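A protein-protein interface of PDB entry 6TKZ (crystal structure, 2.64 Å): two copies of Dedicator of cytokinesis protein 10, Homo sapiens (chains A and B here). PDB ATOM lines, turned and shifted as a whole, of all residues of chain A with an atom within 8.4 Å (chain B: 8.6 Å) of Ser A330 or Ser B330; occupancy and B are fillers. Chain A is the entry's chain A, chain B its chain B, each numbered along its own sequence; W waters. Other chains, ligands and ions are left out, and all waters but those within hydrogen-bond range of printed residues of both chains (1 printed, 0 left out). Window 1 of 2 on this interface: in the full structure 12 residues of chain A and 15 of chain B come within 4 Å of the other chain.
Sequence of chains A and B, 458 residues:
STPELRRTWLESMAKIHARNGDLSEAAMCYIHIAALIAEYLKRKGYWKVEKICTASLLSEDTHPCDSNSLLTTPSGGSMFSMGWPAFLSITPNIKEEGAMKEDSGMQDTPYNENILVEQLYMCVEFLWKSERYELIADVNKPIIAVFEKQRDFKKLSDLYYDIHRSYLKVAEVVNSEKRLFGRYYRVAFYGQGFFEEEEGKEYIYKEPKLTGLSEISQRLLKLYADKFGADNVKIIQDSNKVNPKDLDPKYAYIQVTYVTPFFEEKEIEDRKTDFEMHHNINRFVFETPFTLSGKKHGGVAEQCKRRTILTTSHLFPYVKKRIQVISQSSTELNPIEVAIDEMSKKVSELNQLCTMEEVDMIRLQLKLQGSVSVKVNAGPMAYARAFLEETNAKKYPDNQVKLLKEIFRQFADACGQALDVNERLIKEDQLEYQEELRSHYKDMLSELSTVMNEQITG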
ATOM      1  N   ASN A 240       3.890  24.027 -18.040  1.00  0.00           N
ATOM      2  CA  ASN A 240       3.794  22.878 -17.143  1.00  0.00           C
ATOM      3  C   ASN A 240       4.627  21.726 -17.703  1.00  0.00           C
ATOM      4  O   ASN A 240       4.907  21.659 -18.907  1.00  0.00           O
ATOM      5  CB  ASN A 240       2.329  22.459 -16.955  1.00  0.00           C
ATOM      6  CG  ASN A 240       1.593  23.319 -15.913  1.00  0.00           C
ATOM      7  OD1 ASN A 240       0.658  24.053 -16.253  1.00  0.00           O
ATOM      8  ND2 ASN A 240       2.005  23.209 -14.639  1.00  0.00           N
ATOM      9  N   LYS A 241       5.058  20.828 -16.824  1.00  0.00           N
ATOM     10  CA  LYS A 241       5.822  19.686 -17.311  1.00  0.00           C
ATOM     11  C   LYS A 241       4.983  18.910 -18.318  1.00  0.00           C
ATOM     12  O   LYS A 241       3.802  18.649 -18.083  1.00  0.00           O
ATOM     13  CB  LYS A 241       6.269  18.773 -16.168  1.00  0.00           C
ATOM     14  CG  LYS A 241       7.372  17.811 -16.608  1.00  0.00           C
ATOM     15  CD  LYS A 241       7.528  16.620 -15.673  1.00  0.00           C
ATOM     16  CE  LYS A 241       8.790  15.811 -15.999  1.00  0.00           C
ATOM     17  NZ  LYS A 241      10.034  16.509 -15.565  1.00  0.00           N
ATOM     18  N   PHE A 286      11.087  29.300 -12.705  1.00  0.00           N
ATOM     19  CA  PHE A 286      10.015  29.969 -13.433  1.00  0.00           C
ATOM     20  C   PHE A 286       8.688  29.685 -12.739  1.00  0.00           C
ATOM     21  O   PHE A 286       8.516  28.640 -12.096  1.00  0.00           O
ATOM     22  CB  PHE A 286       9.959  29.533 -14.887  1.00  0.00           C
ATOM     23  CG  PHE A 286       9.616  28.095 -15.073  1.00  0.00           C
ATOM     24  CD1 PHE A 286      10.614  27.126 -15.057  1.00  0.00           C
ATOM     25  CD2 PHE A 286       8.306  27.702 -15.291  1.00  0.00           C
ATOM     26  CE1 PHE A 286      10.302  25.786 -15.242  1.00  0.00           C
ATOM     27  CE2 PHE A 286       7.989  26.362 -15.470  1.00  0.00           C
ATOM     28  CZ  PHE A 286       8.988  25.404 -15.433  1.00  0.00           C
ATOM     29  N   THR A 288       4.443  29.291 -12.995  1.00  0.00           N
ATOM     30  CA  THR A 288       3.328  28.964 -13.882  1.00  0.00           C
ATOM     31  C   THR A 288       2.002  29.277 -13.206  1.00  0.00           C
ATOM     32  O   THR A 288       1.792  28.890 -12.044  1.00  0.00           O
ATOM     33  CB  THR A 288       3.351  27.483 -14.291  1.00  0.00           C
ATOM     34  OG1 THR A 288       4.636  27.165 -14.833  1.00  0.00           O
ATOM     35  CG2 THR A 288       2.278  27.189 -15.352  1.00  0.00           C
ATOM     36  N   PHE A 290      -1.825  28.815 -12.213  1.00  0.00           N
ATOM     37  CA  PHE A 290      -2.972  27.914 -12.221  1.00  0.00           C
ATOM     38  C   PHE A 290      -3.963  28.391 -11.169  1.00  0.00           C
ATOM     39  O   PHE A 290      -3.625  29.195 -10.298  1.00  0.00           O
ATOM     40  CB  PHE A 290      -2.574  26.443 -11.992  1.00  0.00           C
ATOM     41  CG  PHE A 290      -2.141  26.127 -10.584  1.00  0.00           C
ATOM     42  CD1 PHE A 290      -0.853  26.435 -10.150  1.00  0.00           C
ATOM     43  CD2 PHE A 290      -3.011  25.501  -9.697  1.00  0.00           C
ATOM     44  CE1 PHE A 290      -0.440  26.126  -8.840  1.00  0.00           C
ATOM     45  CE2 PHE A 290      -2.623  25.200  -8.400  1.00  0.00           C
ATOM     46  CZ  PHE A 290      -1.330  25.502  -7.967  1.00  0.00           C
ATOM     47  N   LYS A 305      -0.105  29.832  -8.250  1.00  0.00           N
ATOM     48  CA  LYS A 305       1.163  30.032  -8.934  1.00  0.00           C
ATOM     49  C   LYS A 305       2.046  28.853  -8.555  1.00  0.00           C
ATOM     50  O   LYS A 305       2.262  28.610  -7.360  1.00  0.00           O
ATOM     51  CB  LYS A 305       1.778  31.361  -8.491  1.00  0.00           C
ATOM     52  CG  LYS A 305       2.986  31.777  -9.248  1.00  0.00           C
ATOM     53  CD  LYS A 305       3.319  33.252  -9.023  1.00  0.00           C
ATOM     54  CE  LYS A 305       3.830  33.533  -7.615  1.00  0.00           C
ATOM     55  NZ  LYS A 305       4.613  34.806  -7.626  1.00  0.00           N
ATOM     56  N   ARG A 306       2.491  28.084  -9.551  1.00  0.00           N
ATOM     57  CA  ARG A 306       3.484  27.038  -9.339  1.00  0.00           C
ATOM     58  C   ARG A 306       4.872  27.623  -9.574  1.00  0.00           C
ATOM     59  O   ARG A 306       5.090  28.387 -10.521  1.00  0.00           O
ATOM     60  CB  ARG A 306       3.263  25.839 -10.273  1.00  0.00           C
ATOM     61  CG  ARG A 306       3.988  24.524  -9.833  1.00  0.00           C
ATOM     62  CD  ARG A 306       3.743  23.314 -10.783  1.00  0.00           C
ATOM     63  NE  ARG A 306       2.454  23.466 -11.444  1.00  0.00           N
ATOM     64  CZ  ARG A 306       1.307  23.054 -10.933  1.00  0.00           C
ATOM     65  NH1 ARG A 306       1.266  22.324  -9.832  1.00  0.00           N
ATOM     66  NH2 ARG A 306       0.170  23.409 -11.528  1.00  0.00           N
ATOM     67  N   ARG A 307       5.796  27.280  -8.700  1.00  0.00           N
ATOM     68  CA  ARG A 307       7.172  27.743  -8.783  1.00  0.00           C
ATOM     69  C   ARG A 307       8.039  26.509  -8.995  1.00  0.00           C
ATOM     70  O   ARG A 307       8.115  25.643  -8.115  1.00  0.00           O
ATOM     71  CB  ARG A 307       7.557  28.502  -7.515  1.00  0.00           C
ATOM     72  CG  ARG A 307       8.959  29.021  -7.491  1.00  0.00           C
ATOM     73  CD  ARG A 307       9.172  29.878  -6.244  1.00  0.00           C
ATOM     74  NE  ARG A 307       8.443  31.141  -6.326  1.00  0.00           N
ATOM     75  CZ  ARG A 307       8.057  31.838  -5.269  1.00  0.00           C
ATOM     76  NH1 ARG A 307       8.300  31.413  -4.041  1.00  0.00           N
ATOM     77  NH2 ARG A 307       7.414  32.992  -5.446  1.00  0.00           N
ATOM     78  N   THR A 308       8.666  26.418 -10.163  1.00  0.00           N
ATOM     79  CA  THR A 308       9.501  25.281 -10.522  1.00  0.00           C
ATOM     80  C   THR A 308      10.963  25.696 -10.501  1.00  0.00           C
ATOM     81  O   THR A 308      11.328  26.757 -11.020  1.00  0.00           O
ATOM     82  CB  THR A 308       9.177  24.744 -11.921  1.00  0.00           C
ATOM     83  OG1 THR A 308       7.818  24.305 -11.971  1.00  0.00           O
ATOM     84  CG2 THR A 308      10.123  23.584 -12.278  1.00  0.00           C
ATOM     85  N   ILE A 309      11.796  24.836  -9.942  1.00  0.00           N
ATOM     86  CA  ILE A 309      13.215  25.085  -9.842  1.00  0.00           C
ATOM     87  C   ILE A 309      13.923  23.974 -10.595  1.00  0.00           C
ATOM     88  O   ILE A 309      13.852  22.802 -10.196  1.00  0.00           O
ATOM     89  CB  ILE A 309      13.669  25.165  -8.384  1.00  0.00           C
ATOM     90  CG1 ILE A 309      12.843  26.252  -7.670  1.00  0.00           C
ATOM     91  CG2 ILE A 309      15.176  25.469  -8.333  1.00  0.00           C
ATOM     92  CD1 ILE A 309      13.127  26.376  -6.194  1.00  0.00           C
ATOM     93  N   LEU A 310      14.574  24.335 -11.704  1.00  0.00           N
ATOM     94  CA  LEU A 310      15.392  23.425 -12.493  1.00  0.00           C
ATOM     95  C   LEU A 310      16.851  23.499 -12.052  1.00  0.00           C
ATOM     96  O   LEU A 310      17.371  24.582 -11.764  1.00  0.00           O
ATOM     97  CB  LEU A 310      15.278  23.775 -13.970  1.00  0.00           C
ATOM     98  CG  LEU A 310      13.828  23.960 -14.422  1.00  0.00           C
ATOM     99  CD1 LEU A 310      13.765  24.648 -15.743  1.00  0.00           C
ATOM    100  CD2 LEU A 310      13.143  22.613 -14.506  1.00  0.00           C
ATOM    101  N   SER A 327      17.361  17.680 -12.731  1.00  0.00           N
ATOM    102  CA  SER A 327      16.649  17.735 -11.469  1.00  0.00           C
ATOM    103  C   SER A 327      15.600  18.827 -11.577  1.00  0.00           C
ATOM    104  O   SER A 327      15.847  19.869 -12.179  1.00  0.00           O
ATOM    105  CB  SER A 327      17.618  18.018 -10.325  1.00  0.00           C
ATOM    106  OG  SER A 327      16.943  18.598  -9.233  1.00  0.00           O
ATOM    107  N   GLN A 328      14.421  18.574 -11.030  1.00  0.00           N
ATOM    108  CA  GLN A 328      13.485  19.672 -10.862  1.00  0.00           C
ATOM    109  C   GLN A 328      12.667  19.435  -9.602  1.00  0.00           C
ATOM    110  O   GLN A 328      12.394  18.287  -9.232  1.00  0.00           O
ATOM    111  CB  GLN A 328      12.595  19.851 -12.096  1.00  0.00           C
ATOM    112  CG  GLN A 328      11.252  19.182 -12.040  1.00  0.00           C
ATOM    113  CD  GLN A 328      10.259  19.806 -13.040  1.00  0.00           C
ATOM    114  OE1 GLN A 328       9.182  20.257 -12.642  1.00  0.00           O
ATOM    115  NE2 GLN A 328      10.620  19.826 -14.333  1.00  0.00           N
ATOM    116  N   SER A 329      12.358  20.523  -8.908  1.00  0.00           N
ATOM    117  CA  SER A 329      11.437  20.498  -7.783  1.00  0.00           C
ATOM    118  C   SER A 329      10.421  21.611  -7.987  1.00  0.00           C
ATOM    119  O   SER A 329      10.680  22.604  -8.675  1.00  0.00           O
ATOM    120  CB  SER A 329      12.141  20.678  -6.447  1.00  0.00           C
ATOM    121  OG  SER A 329      12.801  21.931  -6.399  1.00  0.00           O
ATOM    122  N   SER A 330       9.241  21.435  -7.420  1.00  0.00           N
ATOM    123  CA  SER A 330       8.235  22.468  -7.573  1.00  0.00           C
ATOM    124  C   SER A 330       7.464  22.603  -6.273  1.00  0.00           C
ATOM    125  O   SER A 330       7.560  21.768  -5.369  1.00  0.00           O
ATOM    126  CB  SER A 330       7.310  22.179  -8.756  1.00  0.00           C
ATOM    127  OG  SER A 330       6.311  21.266  -8.366  1.00  0.00           O
ATOM    128  N   THR A 331       6.720  23.693  -6.182  1.00  0.00           N
ATOM    129  CA  THR A 331       5.960  23.991  -4.984  1.00  0.00           C
ATOM    130  C   THR A 331       4.792  24.864  -5.414  1.00  0.00           C
ATOM    131  O   THR A 331       4.853  25.530  -6.458  1.00  0.00           O
ATOM    132  CB  THR A 331       6.848  24.662  -3.931  1.00  0.00           C
ATOM    133  OG1 THR A 331       6.119  24.802  -2.712  1.00  0.00           O
ATOM    134  CG2 THR A 331       7.304  26.040  -4.394  1.00  0.00           C
ATOM    135  N   GLU A 332       3.702  24.827  -4.657  1.00  0.00           N
ATOM    136  CA  GLU A 332       2.506  25.560  -5.066  1.00  0.00           C
ATOM    137  C   GLU A 332       2.182  26.658  -4.058  1.00  0.00           C
ATOM    138  O   GLU A 332       2.125  26.411  -2.845  1.00  0.00           O
ATOM    139  CB  GLU A 332       1.330  24.617  -5.262  1.00  0.00           C
ATOM    140  CG  GLU A 332       1.455  23.804  -6.541  1.00  0.00           C
ATOM    141  CD  GLU A 332       0.430  22.675  -6.649  1.00  0.00           C
ATOM    142  OE1 GLU A 332      -0.174  22.330  -5.610  1.00  0.00           O
ATOM    143  OE2 GLU A 332       0.252  22.103  -7.761  1.00  0.00           O
ATOM    144  N   LEU A 333       1.993  27.873  -4.572  1.00  0.00           N
ATOM    145  CA  LEU A 333       1.561  29.012  -3.778  1.00  0.00           C
ATOM    146  C   LEU A 333       0.038  29.151  -3.885  1.00  0.00           C
ATOM    147  O   LEU A 333      -0.500  29.270  -5.000  1.00  0.00           O
ATOM    148  CB  LEU A 333       2.273  30.278  -4.249  1.00  0.00           C
ATOM    149  CG  LEU A 333       3.746  30.392  -3.799  1.00  0.00           C
ATOM    150  CD1 LEU A 333       4.746  29.517  -4.594  1.00  0.00           C
ATOM    151  CD2 LEU A 333       4.219  31.860  -3.771  1.00  0.00           C
ATOM    152  N   ASN B 240      17.629  10.726   0.446  1.00  0.00           N
ATOM    153  CA  ASN B 240      17.895  12.031  -0.147  1.00  0.00           C
ATOM    154  C   ASN B 240      19.044  11.941  -1.156  1.00  0.00           C
ATOM    155  O   ASN B 240      19.911  11.062  -1.083  1.00  0.00           O
ATOM    156  CB  ASN B 240      18.260  13.058   0.933  1.00  0.00           C
ATOM    157  CG  ASN B 240      17.049  13.528   1.759  1.00  0.00           C
ATOM    158  OD1 ASN B 240      15.965  13.859   1.221  1.00  0.00           O
ATOM    159  ND2 ASN B 240      17.237  13.564   3.075  1.00  0.00           N
ATOM    160  N   VAL B 285       9.109   6.032  -8.501  1.00  0.00           N
ATOM    161  CA  VAL B 285       8.812   6.948  -7.401  1.00  0.00           C
ATOM    162  C   VAL B 285       9.239   6.329  -6.081  1.00  0.00           C
ATOM    163  O   VAL B 285       9.222   5.108  -5.895  1.00  0.00           O
ATOM    164  CB  VAL B 285       7.315   7.345  -7.322  1.00  0.00           C
ATOM    165  CG1 VAL B 285       6.465   6.140  -7.001  1.00  0.00           C
ATOM    166  CG2 VAL B 285       7.093   8.411  -6.239  1.00  0.00           C
ATOM    167  N   PHE B 286       9.605   7.201  -5.157  1.00  0.00           N
ATOM    168  CA  PHE B 286       9.849   6.833  -3.780  1.00  0.00           C
ATOM    169  C   PHE B 286       9.569   8.063  -2.927  1.00  0.00           C
ATOM    170  O   PHE B 286       9.558   9.193  -3.420  1.00  0.00           O
ATOM    171  CB  PHE B 286      11.279   6.295  -3.589  1.00  0.00           C
ATOM    172  CG  PHE B 286      12.364   7.347  -3.678  1.00  0.00           C
ATOM    173  CD1 PHE B 286      12.770   8.034  -2.542  1.00  0.00           C
ATOM    174  CD2 PHE B 286      13.006   7.626  -4.884  1.00  0.00           C
ATOM    175  CE1 PHE B 286      13.799   8.988  -2.594  1.00  0.00           C
ATOM    176  CE2 PHE B 286      14.038   8.589  -4.949  1.00  0.00           C
ATOM    177  CZ  PHE B 286      14.430   9.265  -3.801  1.00  0.00           C
ATOM    178  N   THR B 288      10.316  10.154   0.895  1.00  0.00           N
ATOM    179  CA  THR B 288      11.323  10.403   1.911  1.00  0.00           C
ATOM    180  C   THR B 288      10.674  11.250   2.999  1.00  0.00           C
ATOM    181  O   THR B 288       9.953  12.221   2.689  1.00  0.00           O
ATOM    182  CB  THR B 288      12.547  11.133   1.347  1.00  0.00           C
ATOM    183  OG1 THR B 288      13.020  10.473   0.165  1.00  0.00           O
ATOM    184  CG2 THR B 288      13.651  11.160   2.371  1.00  0.00           C
ATOM    185  N   PHE B 290      10.598  14.045   5.945  1.00  0.00           N
ATOM    186  CA  PHE B 290      11.320  15.155   6.557  1.00  0.00           C
ATOM    187  C   PHE B 290      10.359  15.972   7.410  1.00  0.00           C
ATOM    188  O   PHE B 290       9.177  16.112   7.086  1.00  0.00           O
ATOM    189  CB  PHE B 290      12.031  16.034   5.502  1.00  0.00           C
ATOM    190  CG  PHE B 290      11.121  16.916   4.684  1.00  0.00           C
ATOM    191  CD1 PHE B 290      10.533  16.442   3.517  1.00  0.00           C
ATOM    192  CD2 PHE B 290      10.893  18.239   5.049  1.00  0.00           C
ATOM    193  CE1 PHE B 290       9.695  17.272   2.747  1.00  0.00           C
ATOM    194  CE2 PHE B 290      10.061  19.069   4.290  1.00  0.00           C
ATOM    195  CZ  PHE B 290       9.465  18.585   3.140  1.00  0.00           C
ATOM    196  N   LYS B 305       6.621  14.853   3.850  1.00  0.00           N
ATOM    197  CA  LYS B 305       7.312  13.848   3.065  1.00  0.00           C
ATOM    198  C   LYS B 305       7.554  14.397   1.670  1.00  0.00           C
ATOM    199  O   LYS B 305       6.776  15.213   1.153  1.00  0.00           O
ATOM    200  CB  LYS B 305       6.536  12.526   3.017  1.00  0.00           C
ATOM    201  CG  LYS B 305       5.274  12.558   2.243  1.00  0.00           C
ATOM    202  CD  LYS B 305       4.590  11.205   2.326  1.00  0.00           C
ATOM    203  CE  LYS B 305       3.359  11.204   1.439  1.00  0.00           C
ATOM    204  NZ  LYS B 305       2.418  10.127   1.767  1.00  0.00           N
ATOM    205  N   ARG B 306       8.666  13.964   1.088  1.00  0.00           N
ATOM    206  CA  ARG B 306       9.041  14.335  -0.267  1.00  0.00           C
ATOM    207  C   ARG B 306       8.740  13.173  -1.203  1.00  0.00           C
ATOM    208  O   ARG B 306       8.921  12.009  -0.841  1.00  0.00           O
ATOM    209  CB  ARG B 306      10.524  14.712  -0.331  1.00  0.00           C
ATOM    210  CG  ARG B 306      11.020  15.200  -1.687  1.00  0.00           C
ATOM    211  CD  ARG B 306      12.466  15.726  -1.576  1.00  0.00           C
ATOM    212  NE  ARG B 306      12.544  16.881  -0.687  1.00  0.00           N
ATOM    213  CZ  ARG B 306      13.096  16.856   0.514  1.00  0.00           C
ATOM    214  NH1 ARG B 306      13.750  15.789   0.948  1.00  0.00           N
ATOM    215  NH2 ARG B 306      12.964  17.919   1.312  1.00  0.00           N
ATOM    216  N   ARG B 307       8.263  13.499  -2.394  1.00  0.00           N
ATOM    217  CA  ARG B 307       7.918  12.534  -3.429  1.00  0.00           C
ATOM    218  C   ARG B 307       8.857  12.769  -4.608  1.00  0.00           C
ATOM    219  O   ARG B 307       8.774  13.807  -5.258  1.00  0.00           O
ATOM    220  CB  ARG B 307       6.460  12.709  -3.842  1.00  0.00           C
ATOM    221  CG  ARG B 307       5.892  11.602  -4.676  1.00  0.00           C
ATOM    222  CD  ARG B 307       4.418  11.845  -4.907  1.00  0.00           C
ATOM    223  NE  ARG B 307       3.656  11.305  -3.781  1.00  0.00           N
ATOM    224  CZ  ARG B 307       2.573  11.870  -3.251  1.00  0.00           C
ATOM    225  NH1 ARG B 307       2.064  12.995  -3.743  1.00  0.00           N
ATOM    226  NH2 ARG B 307       1.974  11.285  -2.214  1.00  0.00           N
ATOM    227  N   THR B 308       9.738  11.806  -4.889  1.00  0.00           N
ATOM    228  CA  THR B 308      10.743  11.915  -5.937  1.00  0.00           C
ATOM    229  C   THR B 308      10.443  10.948  -7.080  1.00  0.00           C
ATOM    230  O   THR B 308      10.151   9.777  -6.843  1.00  0.00           O
ATOM    231  CB  THR B 308      12.127  11.602  -5.377  1.00  0.00           C
ATOM    232  OG1 THR B 308      12.382  12.440  -4.244  1.00  0.00           O
ATOM    233  CG2 THR B 308      13.184  11.826  -6.442  1.00  0.00           C
ATOM    234  N   ILE B 309      10.566  11.405  -8.325  1.00  0.00           N
ATOM    235  CA  ILE B 309      10.307  10.553  -9.478  1.00  0.00           C
ATOM    236  C   ILE B 309      11.542  10.518 -10.386  1.00  0.00           C
ATOM    237  O   ILE B 309      11.910  11.541 -10.987  1.00  0.00           O
ATOM    238  CB  ILE B 309       9.069  11.012 -10.249  1.00  0.00           C
ATOM    239  CG1 ILE B 309       7.835  10.816  -9.353  1.00  0.00           C
ATOM    240  CG2 ILE B 309       8.980  10.270 -11.615  1.00  0.00           C
ATOM    241  CD1 ILE B 309       6.661  11.724  -9.677  1.00  0.00           C
ATOM    242  N   LEU B 310      12.157   9.331 -10.509  1.00  0.00           N
ATOM    243  CA  LEU B 310      13.381   9.122 -11.274  1.00  0.00           C
ATOM    244  C   LEU B 310      13.042   8.678 -12.694  1.00  0.00           C
ATOM    245  O   LEU B 310      12.210   7.790 -12.882  1.00  0.00           O
ATOM    246  CB  LEU B 310      14.277   8.090 -10.563  1.00  0.00           C
ATOM    247  CG  LEU B 310      14.484   8.202  -9.033  1.00  0.00           C
ATOM    248  CD1 LEU B 310      15.239   7.009  -8.433  1.00  0.00           C
ATOM    249  CD2 LEU B 310      15.184   9.520  -8.601  1.00  0.00           C
ATOM    250  N   SER B 327      17.433  12.043 -14.761  1.00  0.00           N
ATOM    251  CA  SER B 327      16.821  13.247 -14.195  1.00  0.00           C
ATOM    252  C   SER B 327      15.889  12.866 -13.056  1.00  0.00           C
ATOM    253  O   SER B 327      15.546  11.697 -12.870  1.00  0.00           O
ATOM    254  CB  SER B 327      16.046  14.044 -15.238  1.00  0.00           C
ATOM    255  OG  SER B 327      15.121  13.188 -15.878  1.00  0.00           O
ATOM    256  N   GLN B 328      15.453  13.892 -12.322  1.00  0.00           N
ATOM    257  CA  GLN B 328      14.619  13.767 -11.131  1.00  0.00           C
ATOM    258  C   GLN B 328      13.612  14.896 -11.082  1.00  0.00           C
ATOM    259  O   GLN B 328      13.966  16.058 -11.309  1.00  0.00           O
ATOM    260  CB  GLN B 328      15.404  13.889  -9.832  1.00  0.00           C
ATOM    261  CG  GLN B 328      16.330  12.820  -9.558  1.00  0.00           C
ATOM    262  CD  GLN B 328      16.765  12.902  -8.139  1.00  0.00           C
ATOM    263  OE1 GLN B 328      16.150  13.626  -7.338  1.00  0.00           O
ATOM    264  NE2 GLN B 328      17.826  12.154  -7.796  1.00  0.00           N
ATOM    265  N   SER B 329      12.392  14.567 -10.683  1.00  0.00           N
ATOM    266  CA  SER B 329      11.408  15.580 -10.350  1.00  0.00           C
ATOM    267  C   SER B 329      10.838  15.275  -8.976  1.00  0.00           C
ATOM    268  O   SER B 329      10.682  14.110  -8.597  1.00  0.00           O
ATOM    269  CB  SER B 329      10.310  15.632 -11.400  1.00  0.00           C
ATOM    270  OG  SER B 329       9.202  14.856 -10.977  1.00  0.00           O
ATOM    271  N   SER B 330      10.550  16.314  -8.208  1.00  0.00           N
ATOM    272  CA  SER B 330      10.114  16.062  -6.850  1.00  0.00           C
ATOM    273  C   SER B 330       9.165  17.158  -6.389  1.00  0.00           C
ATOM    274  O   SER B 330       9.203  18.294  -6.875  1.00  0.00           O
ATOM    275  CB  SER B 330      11.308  15.922  -5.901  1.00  0.00           C
ATOM    276  OG  SER B 330      11.739  17.182  -5.445  1.00  0.00           O
ATOM    277  N   THR B 331       8.282  16.774  -5.477  1.00  0.00           N
ATOM    278  CA  THR B 331       7.272  17.631  -4.887  1.00  0.00           C
ATOM    279  C   THR B 331       7.254  17.323  -3.403  1.00  0.00           C
ATOM    280  O   THR B 331       7.887  16.370  -2.941  1.00  0.00           O
ATOM    281  CB  THR B 331       5.877  17.403  -5.494  1.00  0.00           C
ATOM    282  OG1 THR B 331       5.591  15.998  -5.523  1.00  0.00           O
ATOM    283  CG2 THR B 331       5.796  17.938  -6.905  1.00  0.00           C
ATOM    284  N   GLU B 332       6.536  18.135  -2.647  1.00  0.00           N
ATOM    285  CA  GLU B 332       6.535  17.995  -1.199  1.00  0.00           C
ATOM    286  C   GLU B 332       5.109  18.139  -0.687  1.00  0.00           C
ATOM    287  O   GLU B 332       4.262  18.784  -1.317  1.00  0.00           O
ATOM    288  CB  GLU B 332       7.485  19.029  -0.537  1.00  0.00           C
ATOM    289  CG  GLU B 332       8.974  18.827  -0.882  1.00  0.00           C
ATOM    290  CD  GLU B 332       9.882  19.899  -0.252  1.00  0.00           C
ATOM    291  OE1 GLU B 332       9.351  20.984   0.080  1.00  0.00           O
ATOM    292  OE2 GLU B 332      11.113  19.643  -0.079  1.00  0.00           O
ATOM    293  N   LEU B 333       4.849  17.497   0.443  1.00  0.00           N
ATOM    294  CA  LEU B 333       3.556  17.535   1.109  1.00  0.00           C
ATOM    295  C   LEU B 333       3.789  17.998   2.538  1.00  0.00           C
ATOM    296  O   LEU B 333       4.678  17.472   3.228  1.00  0.00           O
ATOM    297  CB  LEU B 333       2.880  16.160   1.105  1.00  0.00           C
ATOM    298  CG  LEU B 333       2.171  15.637  -0.149  1.00  0.00           C
ATOM    299  CD1 LEU B 333       3.139  15.409  -1.296  1.00  0.00           C
ATOM    300  CD2 LEU B 333       1.444  14.339   0.187  1.00  0.00           C
HETATM  301  O   HOH W   1       5.751  20.689  -3.366  1.00  0.00           O
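Printed residues of chain A that touch a printed residue of chain B: Ser A327, Gln A328, Ser A329 and Ser A330. Of the 18 printed residues of chain B, 4 touch a printed residue of chain A. Among the printed residues, 7 pairs touch across the chains. Among the printed residues, no Asp or Glu carboxylate lies within 4 Å of a Lys or Arg side-chain nitrogen of the other chain.
Printed residues of chain B within 4 Å of Ser A327: Gln B328 (3.2 Å). Of the printed residues of chain B, Gln A328 touches Gln B328, Ser B329 and Ser B330. Of the printed residues of chain B, Ser A329 touches Ser B330. Of chain B, only Ser B330 (3.2 Å) and Thr B331 (3.7 Å) come within 4 Å of Ser A330. No residue of chain B comes within 4 Å of Thr A331. Printed residues of chain A within 4 Å of Gln B328: Ser A327 and Gln A328. Of chain A, only Gln A328, Ser A329 and Ser A330 come within 4 Å of Ser B330. Thr B331 touches just one residue of chain A: Ser A330 (3.7 Å). The nearest residue of chain B that does not touch Ser A330 is Glu B332 (4.7 Å).
Gln B328 touches its own counterpart, Gln A328. Ser A329 touches Ser B330, but with the chains exchanged Ser A330 does not touch Ser B329 (6.6 Å). Ser B330 touches its own counterpart, Ser A330. Ser A330 touches Thr B331, but with the chains exchanged Thr A331 does not touch Ser B330 (6.0 Å). Positions printed for both chains: 240, 286, 288, 290, 305, 306, 307, 308, 309, 310, 327, 328, 329, 330, 331, 332 and 333.
The backbone carbonyl oxygen (O) of Ser B329 sits at hydrogen-bond distance from the backbone NH (N) of Ile B309, 2.7 Å away. O of Thr B331 lies within hydrogen-bond range of N of Arg B307, at 2.9 Å. The backbone NH (N) of Ile A309 sits at hydrogen-bond distance from the backbone carbonyl oxygen (O) of Ser A329 (2.8 Å).
The backbone carbonyl oxygen (O) of Gln B328 is in hydrogen-bond range of the backbone NH (N) of Gln A328 (2.6 Å). O of Ser B330 is in hydrogen-bond range of N of Ser A330 (3.2 Å). The backbone carbonyl oxygen (O) of Gln A328 is in hydrogen-bond range of the backbone NH (N) of Ser B330.
Water W1 lies within hydrogen-bond range of N of Glu B332 and O of Ser A330.
Among the printed residues, pairs that only touch across the chains: Ser A327 with Gln B328, Gln A328 with Ser B329, Ser A329 with Ser B330 and Ser A330 with Thr B331.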
